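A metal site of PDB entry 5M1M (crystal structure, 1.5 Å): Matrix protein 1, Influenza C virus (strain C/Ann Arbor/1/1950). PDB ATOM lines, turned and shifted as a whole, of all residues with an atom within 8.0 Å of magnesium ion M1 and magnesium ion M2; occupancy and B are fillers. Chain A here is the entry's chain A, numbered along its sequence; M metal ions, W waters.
Within 4 Å of magnesium ion M1: Thr 83, Glu 123 and Glu 126.
The nearest printed residue that does not touch magnesium ion M1 is Leu 79 (4.5 Å).
The backbone carbonyl oxygen (O) of Leu 79 sits close to the side-chain hydroxyl (OG1) of Thr 83.
The nearest printed residue that does not touch magnesium ion M2 is Ser 76 (4.2 Å).
Magnesium ion M2 is bound by the side-chain amide oxygen (OD1) of Asn 80 (2.0 Å), water W5 (2.0 Å), the side-chain carboxylate (OD2) of Asp 130 (2.0 Å), the side-chain carboxylate (OE2) of Glu 126 (2.1 Å), water W2 (2.2 Å) and water W4 (2.2 Å).
Magnesium ion M2 has six donor atoms within binding distance.
Water W2 lies within hydrogen-bond range of OD1 of Asp 130 and O of Ser 76.
Water W4 bridges ND2 of Asn 80 (3.4 Å) and OD1 of Asp 130 (3.5 Å).
Magnesium ion M1 is bound by the side-chain carboxylate of Glu 126, water W1, water W6, water W3, the side-chain carboxylate of Glu 123 and the side-chain hydroxyl of Thr 83.
Magnesium ion M1 has six donor atoms within binding distance.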
ATOM      1  N   ALA A  75      28.796  29.747 -34.814  1.00  0.00           N
ATOM      2  CA  ALA A  75      28.061  29.059 -33.750  1.00  0.00           C
ATOM      3  C   ALA A  75      26.773  29.804 -33.424  1.00  0.00           C
ATOM      4  O   ALA A  75      25.708  29.191 -33.259  1.00  0.00           O
ATOM      5  CB  ALA A  75      28.928  28.953 -32.511  1.00  0.00           C
ATOM      6  N   SER A  76      26.890  31.127 -33.343  1.00  0.00           N
ATOM      7  CA  SER A  76      25.749  31.993 -33.054  1.00  0.00           C
ATOM      8  C   SER A  76      24.645  31.806 -34.091  1.00  0.00           C
ATOM      9  O   SER A  76      23.486  31.547 -33.738  1.00  0.00           O
ATOM     10  CB  SER A  76      26.185  33.457 -33.027  1.00  0.00           C
ATOM     11  OG  SER A  76      27.026  33.716 -31.908  1.00  0.00           O
ATOM     12  N   ASP A  77      25.003  31.909 -35.358  1.00  0.00           N
ATOM     13  CA  ASP A  77      24.037  31.783 -36.454  1.00  0.00           C
ATOM     14  C   ASP A  77      23.403  30.397 -36.441  1.00  0.00           C
ATOM     15  O   ASP A  77      22.202  30.275 -36.671  1.00  0.00           O
ATOM     16  CB  ASP A  77      24.718  32.044 -37.813  1.00  0.00           C
ATOM     17  CG  ASP A  77      25.024  33.516 -38.040  1.00  0.00           C
ATOM     18  OD1 ASP A  77      24.485  34.370 -37.319  1.00  0.00           O
ATOM     19  OD2 ASP A  77      25.821  33.807 -38.966  1.00  0.00           O
ATOM     20  N   MET A  78      24.166  29.361 -36.224  1.00  0.00           N
ATOM     21  CA  MET A  78      23.689  28.035 -36.133  1.00  0.00           C
ATOM     22  C   MET A  78      22.576  27.867 -35.083  1.00  0.00           C
ATOM     23  O   MET A  78      21.575  27.277 -35.359  1.00  0.00           O
ATOM     24  CB  MET A  78      24.848  27.112 -35.853  1.00  0.00           C
ATOM     25  CG  MET A  78      24.614  25.637 -35.624  1.00  0.00           C
ATOM     26  SD  MET A  78      23.963  25.066 -34.036  1.00  0.00           S
ATOM     27  CE  MET A  78      25.469  24.920 -33.072  1.00  0.00           C
ATOM     28  N   LEU A  79      22.800  28.392 -33.906  1.00  0.00           N
ATOM     29  CA  LEU A  79      21.799  28.288 -32.838  1.00  0.00           C
ATOM     30  C   LEU A  79      20.528  29.065 -33.173  1.00  0.00           C
ATOM     31  O   LEU A  79      19.422  28.666 -32.789  1.00  0.00           O
ATOM     32  CB  LEU A  79      22.395  28.762 -31.508  1.00  0.00           C
ATOM     33  CG  LEU A  79      23.509  27.854 -30.962  1.00  0.00           C
ATOM     34  CD1 LEU A  79      24.364  28.546 -29.896  1.00  0.00           C
ATOM     35  CD2 LEU A  79      22.894  26.589 -30.397  1.00  0.00           C
ATOM     36  N   ASN A  80      20.681  30.176 -33.896  1.00  0.00           N
ATOM     37  CA  ASN A  80      19.543  30.953 -34.373  1.00  0.00           C
ATOM     38  C   ASN A  80      18.656  30.149 -35.324  1.00  0.00           C
ATOM     39  O   ASN A  80      17.449  30.061 -35.129  1.00  0.00           O
ATOM     40  CB  ASN A  80      20.028  32.216 -35.092  1.00  0.00           C
ATOM     41  CG  ASN A  80      20.621  33.240 -34.160  1.00  0.00           C
ATOM     42  OD1 ASN A  80      20.442  33.156 -32.931  1.00  0.00           O
ATOM     43  ND2 ASN A  80      21.311  34.228 -34.714  1.00  0.00           N
ATOM     44  N   LYS A  81      19.260  29.557 -36.322  1.00  0.00           N
ATOM     45  CA  LYS A  81      18.526  28.786 -37.291  1.00  0.00           C
ATOM     46  C   LYS A  81      17.875  27.561 -36.618  1.00  0.00           C
ATOM     47  O   LYS A  81      16.730  27.239 -36.915  1.00  0.00           O
ATOM     48  CB  LYS A  81      19.462  28.393 -38.427  1.00  0.00           C
ATOM     49  CG  LYS A  81      19.848  29.571 -39.276  1.00  0.00           C
ATOM     50  CD  LYS A  81      18.680  30.176 -40.010  1.00  0.00           C
ATOM     51  CE  LYS A  81      19.027  31.510 -40.587  1.00  0.00           C
ATOM     52  NZ  LYS A  81      19.592  31.439 -41.959  1.00  0.00           N
ATOM     53  N   ALA A  82      18.597  26.907 -35.729  1.00  0.00           N
ATOM     54  CA  ALA A  82      18.117  25.697 -35.050  1.00  0.00           C
ATOM     55  C   ALA A  82      16.925  25.945 -34.121  1.00  0.00           C
ATOM     56  O   ALA A  82      16.261  24.988 -33.697  1.00  0.00           O
ATOM     57  CB  ALA A  82      19.238  25.074 -34.272  1.00  0.00           C
ATOM     58  N   THR A  83      16.668  27.203 -33.793  1.00  0.00           N
ATOM     59  CA  THR A  83      15.553  27.527 -32.899  1.00  0.00           C
ATOM     60  C   THR A  83      14.600  28.555 -33.515  1.00  0.00           C
ATOM     61  O   THR A  83      13.818  29.175 -32.813  1.00  0.00           O
ATOM     62  CB  THR A  83      16.055  28.060 -31.534  1.00  0.00           C
ATOM     63  OG1 THR A  83      16.749  29.302 -31.729  1.00  0.00           O
ATOM     64  CG2 THR A  83      16.976  27.071 -30.874  1.00  0.00           C
ATOM     65  N   SER A  84      14.663  28.710 -34.839  1.00  0.00           N
ATOM     66  CA  SER A  84      13.910  29.783 -35.495  1.00  0.00           C
ATOM     67  C   SER A  84      12.399  29.587 -35.482  1.00  0.00           C
ATOM     68  O   SER A  84      11.649  30.533 -35.702  1.00  0.00           O
ATOM     69  CB  SER A  84      14.402  29.975 -36.936  1.00  0.00           C
ATOM     70  OG  SER A  84      14.075  28.863 -37.742  1.00  0.00           O
ATOM     71  N   SER A  85      11.941  28.367 -35.174  1.00  0.00           N
ATOM     72  CA  SER A  85      10.509  28.078 -35.150  1.00  0.00           C
ATOM     73  C   SER A  85       9.872  28.240 -33.769  1.00  0.00           C
ATOM     74  O   SER A  85       8.679  27.986 -33.594  1.00  0.00           O
ATOM     75  CB  SER A  85      10.239  26.673 -35.684  1.00  0.00           C
ATOM     76  OG  SER A  85      10.662  26.553 -37.032  1.00  0.00           O
ATOM     77  N   LEU A  86      10.669  28.657 -32.773  1.00  0.00           N
ATOM     78  CA  LEU A  86      10.131  28.872 -31.432  1.00  0.00           C
ATOM     79  C   LEU A  86       9.471  30.230 -31.271  1.00  0.00           C
ATOM     80  O   LEU A  86      10.042  31.249 -31.651  1.00  0.00           O
ATOM     81  CB  LEU A  86      11.229  28.720 -30.375  1.00  0.00           C
ATOM     82  CG  LEU A  86      11.699  27.299 -30.078  1.00  0.00           C
ATOM     83  CD1 LEU A  86      12.811  27.292 -29.061  1.00  0.00           C
ATOM     84  CD2 LEU A  86      10.541  26.459 -29.582  1.00  0.00           C
ATOM     85  N   LYS A  87       8.266  30.246 -30.686  1.00  0.00           N
ATOM     86  CA  LYS A  87       7.646  31.505 -30.305  1.00  0.00           C
ATOM     87  C   LYS A  87       8.425  32.113 -29.138  1.00  0.00           C
ATOM     88  O   LYS A  87       9.037  31.387 -28.349  1.00  0.00           O
ATOM     89  CB  LYS A  87       6.179  31.291 -29.909  1.00  0.00           C
ATOM     90  CG  LYS A  87       5.305  30.852 -31.080  1.00  0.00           C
ATOM     91  CD  LYS A  87       3.941  30.351 -30.642  1.00  0.00           C
ATOM     92  CE  LYS A  87       3.077  31.469 -30.109  1.00  0.00           C
ATOM     93  NZ  LYS A  87       1.669  31.304 -30.555  1.00  0.00           N
ATOM     94  N   GLY A  91      10.219  30.462 -25.532  1.00  0.00           N
ATOM     95  CA  GLY A  91      11.558  30.718 -25.034  1.00  0.00           C
ATOM     96  C   GLY A  91      11.545  31.318 -23.642  1.00  0.00           C
ATOM     97  O   GLY A  91      12.410  31.029 -22.819  1.00  0.00           O
ATOM     98  N   ARG A  95      13.544  29.967 -20.407  1.00  0.00           N
ATOM     99  CA  ARG A  95      14.451  30.744 -19.556  1.00  0.00           C
ATOM    100  C   ARG A  95      14.125  30.571 -18.078  1.00  0.00           C
ATOM    101  O   ARG A  95      15.019  30.337 -17.255  1.00  0.00           O
ATOM    102  CB  ARG A  95      14.440  32.226 -19.950  1.00  0.00           C
ATOM    103  CG  ARG A  95      15.043  32.469 -21.325  1.00  0.00           C
ATOM    104  CD  ARG A  95      15.335  33.946 -21.551  1.00  0.00           C
ATOM    105  NE  ARG A  95      14.141  34.790 -21.588  1.00  0.00           N
ATOM    106  CZ  ARG A  95      13.359  34.946 -22.653  1.00  0.00           C
ATOM    107  NH1 ARG A  95      13.597  34.283 -23.774  1.00  0.00           N
ATOM    108  NH2 ARG A  95      12.311  35.750 -22.598  1.00  0.00           N
ATOM    109  N   ASP A 119      14.659  21.341 -30.721  1.00  0.00           N
ATOM    110  CA  ASP A 119      14.726  22.807 -30.811  1.00  0.00           C
ATOM    111  C   ASP A 119      14.640  23.491 -29.428  1.00  0.00           C
ATOM    112  O   ASP A 119      15.222  24.561 -29.221  1.00  0.00           O
ATOM    113  CB  ASP A 119      13.708  23.376 -31.817  1.00  0.00           C
ATOM    114  CG  ASP A 119      12.250  23.195 -31.412  1.00  0.00           C
ATOM    115  OD1 ASP A 119      11.910  22.287 -30.618  1.00  0.00           O
ATOM    116  OD2 ASP A 119      11.421  23.981 -31.908  1.00  0.00           O
ATOM    117  N   MET A 122      17.864  23.121 -27.754  1.00  0.00           N
ATOM    118  CA  MET A 122      18.843  23.969 -28.391  1.00  0.00           C
ATOM    119  C   MET A 122      18.707  25.440 -28.054  1.00  0.00           C
ATOM    120  O   MET A 122      19.660  26.165 -28.073  1.00  0.00           O
ATOM    121  CB  MET A 122      18.846  23.715 -29.920  1.00  0.00           C
ATOM    122  CG  MET A 122      19.323  22.273 -30.328  1.00  0.00           C
ATOM    123  SD  MET A 122      21.032  22.052 -29.724  1.00  0.00           S
ATOM    124  CE  MET A 122      21.640  23.245 -30.827  1.00  0.00           C
ATOM    125  N   GLU A 123      17.470  25.756 -27.726  1.00  0.00           N
ATOM    126  CA  GLU A 123      17.199  27.077 -27.174  1.00  0.00           C
ATOM    127  C   GLU A 123      17.843  27.277 -25.799  1.00  0.00           C
ATOM    128  O   GLU A 123      18.269  28.380 -25.458  1.00  0.00           O
ATOM    129  CB  GLU A 123      15.683  27.281 -27.105  1.00  0.00           C
ATOM    130  CG  GLU A 123      15.243  28.656 -26.583  1.00  0.00           C
ATOM    131  CD  GLU A 123      15.393  29.788 -27.589  1.00  0.00           C
ATOM    132  OE1 GLU A 123      15.876  29.567 -28.730  1.00  0.00           O
ATOM    133  OE2 GLU A 123      15.003  30.929 -27.248  1.00  0.00           O
ATOM    134  N   MET A 124      17.914  26.205 -25.010  1.00  0.00           N
ATOM    135  CA  MET A 124      18.651  26.243 -23.740  1.00  0.00           C
ATOM    136  C   MET A 124      20.137  26.489 -24.011  1.00  0.00           C
ATOM    137  O   MET A 124      20.781  27.317 -23.348  1.00  0.00           O
ATOM    138  CB  MET A 124      18.479  24.940 -22.960  1.00  0.00           C
ATOM    139  CG  MET A 124      17.033  24.660 -22.544  1.00  0.00           C
ATOM    140  SD  MET A 124      16.878  23.008 -21.840  1.00  0.00           S
ATOM    141  CE  MET A 124      17.754  23.239 -20.312  1.00  0.00           C
ATOM    142  N   GLU A 126      21.395  27.905 -26.680  1.00  0.00           N
ATOM    143  CA  GLU A 126      21.508  29.262 -27.205  1.00  0.00           C
ATOM    144  C   GLU A 126      21.459  30.290 -26.081  1.00  0.00           C
ATOM    145  O   GLU A 126      22.184  31.294 -26.103  1.00  0.00           O
ATOM    146  CB  GLU A 126      20.393  29.566 -28.195  1.00  0.00           C
ATOM    147  CG  GLU A 126      20.587  30.912 -28.864  1.00  0.00           C
ATOM    148  CD  GLU A 126      19.412  31.308 -29.729  1.00  0.00           C
ATOM    149  OE1 GLU A 126      18.357  30.636 -29.674  1.00  0.00           O
ATOM    150  OE2 GLU A 126      19.552  32.312 -30.457  1.00  0.00           O
ATOM    151  N   GLU A 127      20.587  30.074 -25.107  1.00  0.00           N
ATOM    152  CA  GLU A 127      20.552  30.954 -23.934  1.00  0.00           C
ATOM    153  C   GLU A 127      21.915  31.056 -23.250  1.00  0.00           C
ATOM    154  O   GLU A 127      22.396  32.152 -22.976  1.00  0.00           O
ATOM    155  CB  GLU A 127      19.459  30.502 -22.950  1.00  0.00           C
ATOM    156  CG  GLU A 127      18.095  31.086 -23.240  1.00  0.00           C
ATOM    157  CD  GLU A 127      18.098  32.606 -23.287  1.00  0.00           C
ATOM    158  OE1 GLU A 127      18.584  33.241 -22.327  1.00  0.00           O
ATOM    159  OE2 GLU A 127      17.634  33.173 -24.305  1.00  0.00           O
ATOM    160  N   TYR A 129      24.880  30.282 -24.574  1.00  0.00           N
ATOM    161  CA  TYR A 129      25.907  30.782 -25.492  1.00  0.00           C
ATOM    162  C   TYR A 129      25.756  32.255 -25.855  1.00  0.00           C
ATOM    163  O   TYR A 129      26.734  32.998 -25.915  1.00  0.00           O
ATOM    164  CB  TYR A 129      25.951  29.951 -26.778  1.00  0.00           C
ATOM    165  CG  TYR A 129      27.157  30.233 -27.665  1.00  0.00           C
ATOM    166  CD1 TYR A 129      28.428  29.818 -27.294  1.00  0.00           C
ATOM    167  CD2 TYR A 129      27.011  30.921 -28.858  1.00  0.00           C
ATOM    168  CE1 TYR A 129      29.536  30.053 -28.122  1.00  0.00           C
ATOM    169  CE2 TYR A 129      28.115  31.171 -29.669  1.00  0.00           C
ATOM    170  CZ  TYR A 129      29.356  30.750 -29.292  1.00  0.00           C
ATOM    171  OH  TYR A 129      30.422  30.993 -30.128  1.00  0.00           O
ATOM    172  N   ASP A 130      24.509  32.689 -26.077  1.00  0.00           N
ATOM    173  CA  ASP A 130      24.226  34.075 -26.448  1.00  0.00           C
ATOM    174  C   ASP A 130      24.262  34.968 -25.214  1.00  0.00           C
ATOM    175  O   ASP A 130      24.688  36.122 -25.283  1.00  0.00           O
ATOM    176  CB  ASP A 130      22.827  34.196 -27.076  1.00  0.00           C
ATOM    177  CG  ASP A 130      22.791  33.787 -28.548  1.00  0.00           C
ATOM    178  OD1 ASP A 130      23.802  33.271 -29.089  1.00  0.00           O
ATOM    179  OD2 ASP A 130      21.707  33.968 -29.160  1.00  0.00           O
ATOM    180  N   HIS A 131      23.778  34.429 -24.102  1.00  0.00           N
ATOM    181  CA  HIS A 131      23.649  35.216 -22.866  1.00  0.00           C
ATOM    182  C   HIS A 131      24.227  34.528 -21.619  1.00  0.00           C
ATOM    183  O   HIS A 131      23.530  34.387 -20.595  1.00  0.00           O
ATOM    184  CB  HIS A 131      22.175  35.565 -22.628  1.00  0.00           C
ATOM    185  CG  HIS A 131      21.508  36.187 -23.821  1.00  0.00           C
ATOM    186  ND1 HIS A 131      21.755  37.479 -24.223  1.00  0.00           N
ATOM    187  CD2 HIS A 131      20.618  35.677 -24.711  1.00  0.00           C
ATOM    188  CE1 HIS A 131      21.050  37.743 -25.302  1.00  0.00           C
ATOM    189  NE2 HIS A 131      20.357  36.681 -25.625  1.00  0.00           N
HETATM  190 MG    MG M   1      16.447  30.961 -30.321  1.00  0.00          MG
HETATM  191 MG    MG M   2      21.016  33.648 -31.062  1.00  0.00          MG
HETATM  192  O   HOH W   1      14.550  31.040 -31.099  1.00  0.00           O
HETATM  193  O   HOH W   2      22.623  32.222 -31.239  1.00  0.00           O
HETATM  194  O   HOH W   3      16.029  32.587 -29.078  1.00  0.00           O
HETATM  195  O   HOH W   4      22.454  35.141 -31.696  1.00  0.00           O
HETATM  196  O   HOH W   5      19.660  35.147 -30.940  1.00  0.00           O
HETATM  197  O   HOH W   6      17.266  32.218 -31.736  1.00  0.00           O
